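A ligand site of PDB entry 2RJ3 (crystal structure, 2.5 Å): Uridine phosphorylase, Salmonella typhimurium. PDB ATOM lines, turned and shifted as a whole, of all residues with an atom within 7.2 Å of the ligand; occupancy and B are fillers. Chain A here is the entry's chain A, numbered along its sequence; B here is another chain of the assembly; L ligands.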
ATOM      1  N   ILE A  68     -18.585  14.787 -35.511  1.00  0.00           N
ATOM      2  CA  ILE A  68     -19.310  13.530 -35.341  1.00  0.00           C
ATOM      3  C   ILE A  68     -19.914  13.067 -36.659  1.00  0.00           C
ATOM      4  O   ILE A  68     -20.594  13.851 -37.338  1.00  0.00           O
ATOM      5  CB  ILE A  68     -20.431  13.628 -34.288  1.00  0.00           C
ATOM      6  CG1 ILE A  68     -19.853  13.897 -32.903  1.00  0.00           C
ATOM      7  CG2 ILE A  68     -21.282  12.357 -34.287  1.00  0.00           C
ATOM      8  CD1 ILE A  68     -20.860  14.454 -31.905  1.00  0.00           C
ATOM      9  N   ARG A  90      -7.369   7.467 -36.153  1.00  0.00           N
ATOM     10  CA  ARG A  90      -8.543   7.896 -35.418  1.00  0.00           C
ATOM     11  C   ARG A  90      -8.348   7.624 -33.939  1.00  0.00           C
ATOM     12  O   ARG A  90      -8.091   6.490 -33.533  1.00  0.00           O
ATOM     13  CB  ARG A  90      -9.787   7.152 -35.914  1.00  0.00           C
ATOM     14  CG  ARG A  90     -11.024   8.010 -36.133  1.00  0.00           C
ATOM     15  CD  ARG A  90     -11.593   8.590 -34.849  1.00  0.00           C
ATOM     16  NE  ARG A  90     -12.759   7.880 -34.344  1.00  0.00           N
ATOM     17  CZ  ARG A  90     -13.718   8.449 -33.622  1.00  0.00           C
ATOM     18  NH1 ARG A  90     -13.668   9.746 -33.343  1.00  0.00           N
ATOM     19  NH2 ARG A  90     -14.746   7.734 -33.171  1.00  0.00           N
ATOM     20  N   GLY A  92     -10.751   8.243 -30.659  1.00  0.00           N
ATOM     21  CA  GLY A  92     -12.117   8.611 -30.276  1.00  0.00           C
ATOM     22  C   GLY A  92     -12.534   8.184 -28.871  1.00  0.00           C
ATOM     23  O   GLY A  92     -11.729   7.653 -28.114  1.00  0.00           O
ATOM     24  N   THR A  93     -13.789   8.446 -28.537  1.00  0.00           N
ATOM     25  CA  THR A  93     -14.414   7.919 -27.322  1.00  0.00           C
ATOM     26  C   THR A  93     -15.498   6.930 -27.745  1.00  0.00           C
ATOM     27  O   THR A  93     -16.040   7.025 -28.850  1.00  0.00           O
ATOM     28  CB  THR A  93     -15.013   9.022 -26.415  1.00  0.00           C
ATOM     29  OG1 THR A  93     -15.993   9.773 -27.152  1.00  0.00           O
ATOM     30  CG2 THR A  93     -13.922   9.957 -25.899  1.00  0.00           C
ATOM     31  N   THR A  94     -15.808   5.983 -26.867  1.00  0.00           N
ATOM     32  CA  THR A  94     -16.679   4.873 -27.233  1.00  0.00           C
ATOM     33  C   THR A  94     -17.496   4.333 -26.054  1.00  0.00           C
ATOM     34  O   THR A  94     -17.163   4.565 -24.894  1.00  0.00           O
ATOM     35  CB  THR A  94     -15.866   3.727 -27.905  1.00  0.00           C
ATOM     36  OG1 THR A  94     -16.758   2.701 -28.349  1.00  0.00           O
ATOM     37  CG2 THR A  94     -14.837   3.120 -26.944  1.00  0.00           C
ATOM     38  N   GLY A  95     -18.576   3.630 -26.383  1.00  0.00           N
ATOM     39  CA  GLY A  95     -19.353   2.908 -25.401  1.00  0.00           C
ATOM     40  C   GLY A  95     -19.117   1.423 -25.557  1.00  0.00           C
ATOM     41  O   GLY A  95     -19.452   0.828 -26.591  1.00  0.00           O
ATOM     42  N   ALA A  96     -18.510   0.807 -24.534  1.00  0.00           N
ATOM     43  CA  ALA A  96     -18.245  -0.622 -24.551  1.00  0.00           C
ATOM     44  C   ALA A  96     -19.537  -1.397 -24.334  1.00  0.00           C
ATOM     45  O   ALA A  96     -20.426  -0.945 -23.603  1.00  0.00           O
ATOM     46  CB  ALA A  96     -17.217  -0.994 -23.485  1.00  0.00           C
ATOM     47  N   ALA A 156     -18.809  -1.716 -33.660  1.00  0.00           N
ATOM     48  CA  ALA A 156     -20.039  -1.280 -34.305  1.00  0.00           C
ATOM     49  C   ALA A 156     -19.984   0.222 -34.547  1.00  0.00           C
ATOM     50  O   ALA A 156     -19.972   1.013 -33.592  1.00  0.00           O
ATOM     51  CB  ALA A 156     -21.245  -1.656 -33.455  1.00  0.00           C
ATOM     52  N   SER A 158     -21.901   3.284 -35.852  1.00  0.00           N
ATOM     53  CA  SER A 158     -23.289   3.681 -36.100  1.00  0.00           C
ATOM     54  C   SER A 158     -23.457   5.130 -36.524  1.00  0.00           C
ATOM     55  O   SER A 158     -22.778   6.026 -36.000  1.00  0.00           O
ATOM     56  CB  SER A 158     -24.138   3.411 -34.844  1.00  0.00           C
ATOM     57  OG  SER A 158     -25.336   4.149 -34.866  1.00  0.00           O
ATOM     58  N   THR A 160     -25.993   6.875 -35.827  1.00  0.00           N
ATOM     59  CA  THR A 160     -26.676   7.585 -34.745  1.00  0.00           C
ATOM     60  C   THR A 160     -26.088   7.250 -33.374  1.00  0.00           C
ATOM     61  O   THR A 160     -25.537   6.163 -33.167  1.00  0.00           O
ATOM     62  CB  THR A 160     -28.207   7.343 -34.706  1.00  0.00           C
ATOM     63  OG1 THR A 160     -28.480   5.934 -34.658  1.00  0.00           O
ATOM     64  CG2 THR A 160     -28.887   7.966 -35.918  1.00  0.00           C
ATOM     65  N   PHE A 161     -26.221   8.202 -32.455  1.00  0.00           N
ATOM     66  CA  PHE A 161     -25.818   8.018 -31.061  1.00  0.00           C
ATOM     67  C   PHE A 161     -26.893   7.249 -30.302  1.00  0.00           C
ATOM     68  O   PHE A 161     -26.606   6.579 -29.310  1.00  0.00           O
ATOM     69  CB  PHE A 161     -25.590   9.391 -30.410  1.00  0.00           C
ATOM     70  CG  PHE A 161     -25.034   9.313 -29.004  1.00  0.00           C
ATOM     71  CD1 PHE A 161     -25.882   9.305 -27.903  1.00  0.00           C
ATOM     72  CD2 PHE A 161     -23.660   9.270 -28.795  1.00  0.00           C
ATOM     73  CE1 PHE A 161     -25.371   9.240 -26.605  1.00  0.00           C
ATOM     74  CE2 PHE A 161     -23.135   9.205 -27.502  1.00  0.00           C
ATOM     75  CZ  PHE A 161     -23.999   9.188 -26.401  1.00  0.00           C
ATOM     76  N   GLN A 165     -27.657   2.660 -31.752  1.00  0.00           N
ATOM     77  CA  GLN A 165     -26.918   2.076 -30.636  1.00  0.00           C
ATOM     78  C   GLN A 165     -27.924   1.591 -29.598  1.00  0.00           C
ATOM     79  O   GLN A 165     -27.604   1.474 -28.413  1.00  0.00           O
ATOM     80  CB  GLN A 165     -25.965   3.107 -30.017  1.00  0.00           C
ATOM     81  CG  GLN A 165     -24.907   3.626 -30.972  1.00  0.00           C
ATOM     82  CD  GLN A 165     -23.871   4.476 -30.277  1.00  0.00           C
ATOM     83  OE1 GLN A 165     -23.657   4.376 -29.075  1.00  0.00           O
ATOM     84  NE2 GLN A 165     -23.209   5.335 -31.051  1.00  0.00           N
ATOM     85  N   ARG A 167     -30.307   2.845 -27.894  1.00  0.00           N
ATOM     86  CA  ARG A 167     -30.654   3.642 -26.722  1.00  0.00           C
ATOM     87  C   ARG A 167     -32.154   3.911 -26.731  1.00  0.00           C
ATOM     88  O   ARG A 167     -32.721   4.225 -27.777  1.00  0.00           O
ATOM     89  CB  ARG A 167     -29.868   4.966 -26.704  1.00  0.00           C
ATOM     90  CG  ARG A 167     -28.463   4.841 -26.150  1.00  0.00           C
ATOM     91  CD  ARG A 167     -27.779   6.190 -26.085  1.00  0.00           C
ATOM     92  NE  ARG A 167     -26.569   6.155 -25.268  1.00  0.00           N
ATOM     93  CZ  ARG A 167     -25.339   5.919 -25.743  1.00  0.00           C
ATOM     94  NH1 ARG A 167     -25.147   5.707 -27.033  1.00  0.00           N
ATOM     95  NH2 ARG A 167     -24.309   5.896 -24.906  1.00  0.00           N
ATOM     96  N   ASN A 193     -17.698  -2.638 -28.958  1.00  0.00           N
ATOM     97  CA  ASN A 193     -18.065  -1.242 -28.731  1.00  0.00           C
ATOM     98  C   ASN A 193     -18.854  -0.519 -29.821  1.00  0.00           C
ATOM     99  O   ASN A 193     -18.882  -0.949 -30.975  1.00  0.00           O
ATOM    100  CB  ASN A 193     -16.797  -0.426 -28.440  1.00  0.00           C
ATOM    101  CG  ASN A 193     -15.812  -0.455 -29.598  1.00  0.00           C
ATOM    102  OD1 ASN A 193     -15.615  -1.491 -30.227  1.00  0.00           O
ATOM    103  ND2 ASN A 193     -15.195   0.681 -29.881  1.00  0.00           N
ATOM    104  N   TYR A 194     -19.484   0.588 -29.438  1.00  0.00           N
ATOM    105  CA  TYR A 194     -20.141   1.511 -30.356  1.00  0.00           C
ATOM    106  C   TYR A 194     -19.347   2.807 -30.480  1.00  0.00           C
ATOM    107  O   TYR A 194     -18.973   3.415 -29.466  1.00  0.00           O
ATOM    108  CB  TYR A 194     -21.543   1.898 -29.863  1.00  0.00           C
ATOM    109  CG  TYR A 194     -22.662   0.883 -30.033  1.00  0.00           C
ATOM    110  CD1 TYR A 194     -23.117   0.521 -31.306  1.00  0.00           C
ATOM    111  CD2 TYR A 194     -23.316   0.352 -28.924  1.00  0.00           C
ATOM    112  CE1 TYR A 194     -24.171  -0.392 -31.458  1.00  0.00           C
ATOM    113  CE2 TYR A 194     -24.372  -0.557 -29.063  1.00  0.00           C
ATOM    114  CZ  TYR A 194     -24.787  -0.922 -30.325  1.00  0.00           C
ATOM    115  OH  TYR A 194     -25.825  -1.814 -30.459  1.00  0.00           O
ATOM    116  N   GLU A 195     -19.081   3.212 -31.713  1.00  0.00           N
ATOM    117  CA  GLU A 195     -18.670   4.596 -32.010  1.00  0.00           C
ATOM    118  C   GLU A 195     -19.329   5.049 -33.327  1.00  0.00           C
ATOM    119  O   GLU A 195     -20.189   4.348 -33.845  1.00  0.00           O
ATOM    120  CB  GLU A 195     -17.139   4.745 -31.987  1.00  0.00           C
ATOM    121  CG  GLU A 195     -16.386   3.867 -32.946  1.00  0.00           C
ATOM    122  CD  GLU A 195     -16.244   4.486 -34.317  1.00  0.00           C
ATOM    123  OE1 GLU A 195     -15.434   5.427 -34.463  1.00  0.00           O
ATOM    124  OE2 GLU A 195     -16.946   4.032 -35.246  1.00  0.00           O
ATOM    125  N   MET A 196     -18.932   6.204 -33.860  1.00  0.00           N
ATOM    126  CA  MET A 196     -19.696   6.812 -34.944  1.00  0.00           C
ATOM    127  C   MET A 196     -18.968   7.223 -36.229  1.00  0.00           C
ATOM    128  O   MET A 196     -19.579   7.845 -37.091  1.00  0.00           O
ATOM    129  CB  MET A 196     -20.495   8.011 -34.416  1.00  0.00           C
ATOM    130  CG  MET A 196     -21.533   7.644 -33.362  1.00  0.00           C
ATOM    131  SD  MET A 196     -22.545   9.037 -32.897  1.00  0.00           S
ATOM    132  CE  MET A 196     -23.475   9.310 -34.401  1.00  0.00           C
ATOM    133  N   GLU A 197     -17.691   6.874 -36.374  1.00  0.00           N
ATOM    134  CA  GLU A 197     -16.999   7.240 -37.625  1.00  0.00           C
ATOM    135  C   GLU A 197     -15.964   6.256 -38.184  1.00  0.00           C
ATOM    136  O   GLU A 197     -15.393   6.511 -39.244  1.00  0.00           O
ATOM    137  CB  GLU A 197     -16.426   8.669 -37.571  1.00  0.00           C
ATOM    138  CG  GLU A 197     -15.847   9.117 -36.237  1.00  0.00           C
ATOM    139  CD  GLU A 197     -16.904   9.621 -35.267  1.00  0.00           C
ATOM    140  OE1 GLU A 197     -16.958   9.101 -34.136  1.00  0.00           O
ATOM    141  OE2 GLU A 197     -17.690  10.520 -35.641  1.00  0.00           O
ATOM    142  N   GLY A 217     -11.112   5.384 -26.376  1.00  0.00           N
ATOM    143  CA  GLY A 217     -11.163   5.191 -24.927  1.00  0.00           C
ATOM    144  C   GLY A 217     -12.587   4.975 -24.455  1.00  0.00           C
ATOM    145  O   GLY A 217     -13.477   5.734 -24.825  1.00  0.00           O
ATOM    146  N   ILE A 219     -15.626   5.324 -22.361  1.00  0.00           N
ATOM    147  CA  ILE A 219     -16.187   6.308 -21.429  1.00  0.00           C
ATOM    148  C   ILE A 219     -17.469   5.815 -20.734  1.00  0.00           C
ATOM    149  O   ILE A 219     -17.862   6.356 -19.693  1.00  0.00           O
ATOM    150  CB  ILE A 219     -16.440   7.684 -22.105  1.00  0.00           C
ATOM    151  CG1 ILE A 219     -17.398   7.556 -23.293  1.00  0.00           C
ATOM    152  CG2 ILE A 219     -15.112   8.315 -22.520  1.00  0.00           C
ATOM    153  CD1 ILE A 219     -17.977   8.886 -23.778  1.00  0.00           C
ATOM    154  N   VAL A 220     -18.091   4.793 -21.311  1.00  0.00           N
ATOM    155  CA  VAL A 220     -19.277   4.161 -20.725  1.00  0.00           C
ATOM    156  C   VAL A 220     -19.328   2.672 -21.081  1.00  0.00           C
ATOM    157  O   VAL A 220     -18.831   2.246 -22.125  1.00  0.00           O
ATOM    158  CB  VAL A 220     -20.594   4.910 -21.136  1.00  0.00           C
ATOM    159  CG1 VAL A 220     -20.946   4.708 -22.616  1.00  0.00           C
ATOM    160  CG2 VAL A 220     -21.780   4.493 -20.241  1.00  0.00           C
ATOM    161  N   ASN A 221     -19.896   1.879 -20.173  1.00  0.00           N
ATOM    162  CA  ASN A 221     -20.242   0.492 -20.469  1.00  0.00           C
ATOM    163  C   ASN A 221     -21.746   0.312 -20.364  1.00  0.00           C
ATOM    164  O   ASN A 221     -22.352   0.621 -19.335  1.00  0.00           O
ATOM    165  CB  ASN A 221     -19.493  -0.473 -19.537  1.00  0.00           C
ATOM    166  CG  ASN A 221     -19.611  -1.915 -19.989  1.00  0.00           C
ATOM    167  OD1 ASN A 221     -20.665  -2.546 -19.867  1.00  0.00           O
ATOM    168  ND2 ASN A 221     -18.523  -2.463 -20.513  1.00  0.00           N
ATOM    169  N   ARG A 222     -22.336  -0.208 -21.437  1.00  0.00           N
ATOM    170  CA  ARG A 222     -23.791  -0.316 -21.570  1.00  0.00           C
ATOM    171  C   ARG A 222     -24.404  -1.456 -20.754  1.00  0.00           C
ATOM    172  O   ARG A 222     -25.630  -1.559 -20.661  1.00  0.00           O
ATOM    173  CB  ARG A 222     -24.186  -0.430 -23.041  1.00  0.00           C
ATOM    174  CG  ARG A 222     -23.829   0.785 -23.895  1.00  0.00           C
ATOM    175  CD  ARG A 222     -24.825   1.930 -23.730  1.00  0.00           C
ATOM    176  NE  ARG A 222     -26.170   1.530 -24.124  1.00  0.00           N
ATOM    177  CZ  ARG A 222     -26.630   1.568 -25.376  1.00  0.00           C
ATOM    178  NH1 ARG A 222     -25.852   1.991 -26.367  1.00  0.00           N
ATOM    179  NH2 ARG A 222     -27.865   1.177 -25.626  1.00  0.00           N
ATOM    180  N   PHE B   6     -26.684  15.260 -23.467  1.00  0.00           N
ATOM    181  CA  PHE B   6     -25.297  14.778 -23.488  1.00  0.00           C
ATOM    182  C   PHE B   6     -24.304  15.623 -24.303  1.00  0.00           C
ATOM    183  O   PHE B   6     -23.139  15.698 -23.938  1.00  0.00           O
ATOM    184  CB  PHE B   6     -25.255  13.312 -23.926  1.00  0.00           C
ATOM    185  CG  PHE B   6     -23.929  12.637 -23.654  1.00  0.00           C
ATOM    186  CD1 PHE B   6     -23.640  12.138 -22.381  1.00  0.00           C
ATOM    187  CD2 PHE B   6     -22.966  12.518 -24.663  1.00  0.00           C
ATOM    188  CE1 PHE B   6     -22.412  11.518 -22.121  1.00  0.00           C
ATOM    189  CE2 PHE B   6     -21.742  11.905 -24.415  1.00  0.00           C
ATOM    190  CZ  PHE B   6     -21.468  11.399 -23.142  1.00  0.00           C
ATOM    191  N   HIS B   7     -24.764  16.254 -25.379  1.00  0.00           N
ATOM    192  CA  HIS B   7     -23.855  16.905 -26.335  1.00  0.00           C
ATOM    193  C   HIS B   7     -23.946  18.440 -26.442  1.00  0.00           C
ATOM    194  O   HIS B   7     -22.949  19.098 -26.712  1.00  0.00           O
ATOM    195  CB  HIS B   7     -24.022  16.303 -27.728  1.00  0.00           C
ATOM    196  CG  HIS B   7     -23.606  14.870 -27.828  1.00  0.00           C
ATOM    197  ND1 HIS B   7     -24.499  13.823 -27.664  1.00  0.00           N
ATOM    198  CD2 HIS B   7     -22.404  14.296 -28.084  1.00  0.00           C
ATOM    199  CE1 HIS B   7     -23.860  12.681 -27.821  1.00  0.00           C
ATOM    200  NE2 HIS B   7     -22.589  12.942 -28.071  1.00  0.00           N
ATOM    201  N   ARG B  47     -18.578  20.993 -29.237  1.00  0.00           N
ATOM    202  CA  ARG B  47     -18.272  20.320 -30.508  1.00  0.00           C
ATOM    203  C   ARG B  47     -18.758  21.186 -31.679  1.00  0.00           C
ATOM    204  O   ARG B  47     -18.458  22.386 -31.720  1.00  0.00           O
ATOM    205  CB  ARG B  47     -18.844  18.889 -30.539  1.00  0.00           C
ATOM    206  CG  ARG B  47     -18.123  17.903 -29.620  1.00  0.00           C
ATOM    207  CD  ARG B  47     -18.901  16.599 -29.489  1.00  0.00           C
ATOM    208  NE  ARG B  47     -18.149  15.528 -28.832  1.00  0.00           N
ATOM    209  CZ  ARG B  47     -17.447  14.593 -29.474  1.00  0.00           C
ATOM    210  NH1 ARG B  47     -17.381  14.584 -30.797  1.00  0.00           N
ATOM    211  NH2 ARG B  47     -16.794  13.668 -28.782  1.00  0.00           N
HETATM  212  N1  LIG L   1     -19.524   7.372 -28.238  1.00  0.00           N
HETATM  213  C1  LIG L   1     -20.484   6.653 -28.848  1.00  0.00           C
HETATM  214  O1  LIG L   1     -20.571   6.679 -30.101  1.00  0.00           O
HETATM  215  N2  LIG L   1     -21.341   5.902 -28.136  1.00  0.00           N
HETATM  216  C2  LIG L   1     -21.264   5.855 -26.798  1.00  0.00           C
HETATM  217  O2  LIG L   1     -22.066   5.162 -26.152  1.00  0.00           O
HETATM  218  C3  LIG L   1     -20.277   6.597 -26.138  1.00  0.00           C
HETATM  219  C4  LIG L   1     -19.406   7.360 -26.899  1.00  0.00           C
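OE1 of Gln 165 is in hydrogen-bond range of N2 of the ligand (2.9 Å).
An oxygen (O2) of the ligand sits at hydrogen-bond distance from the guanidinium group of Arg 167, 2.7 Å away.
O of Thr 160 sits at hydrogen-bond distance from NE2 of Gln 165.
O of Glu 195 lies within hydrogen-bond range of N of Ser 158 (2.8 Å).
O of Gly 95 lies within hydrogen-bond range of N of Tyr 194, at 2.9 Å.
NH1 of Arg 167 sits at hydrogen-bond distance from O of Phe 161.
The backbone carbonyl oxygen of Thr 94 sits at hydrogen-bond distance from the backbone NH of Ile 219 (3.1 Å).
The side-chain carboxylate of Glu 195 lies within hydrogen-bond range of the backbone NH of Glu 197 (3.1 Å).
The guanidinium group of Arg 222 sits at hydrogen-bond distance from the backbone carbonyl oxygen of Gln 165, at 2.7 Å.
The side-chain amide oxygen (OE1) of Gln 165 is in hydrogen-bond range of the guanidinium group (NH1) of Arg 167 (2.9 Å).
Merely in contact with the ligand: Glu 195 (3.4 Å), Gly 95 (3.4 Å), Met 196 (3.5 Å), Thr 93 (3.6 Å), Thr 94 (3.6 Å), Tyr 194 (3.6 Å), Val 220 (3.7 Å), Ile 219 (3.8 Å) and Phe 161 (3.8 Å).
Hydrophobic or aromatic side chains that line the ligand: Phe 161, Met 196, Ile 219 and Val 220.
The nearest printed residue that does not touch the ligand is Arg 222 (4.9 Å).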
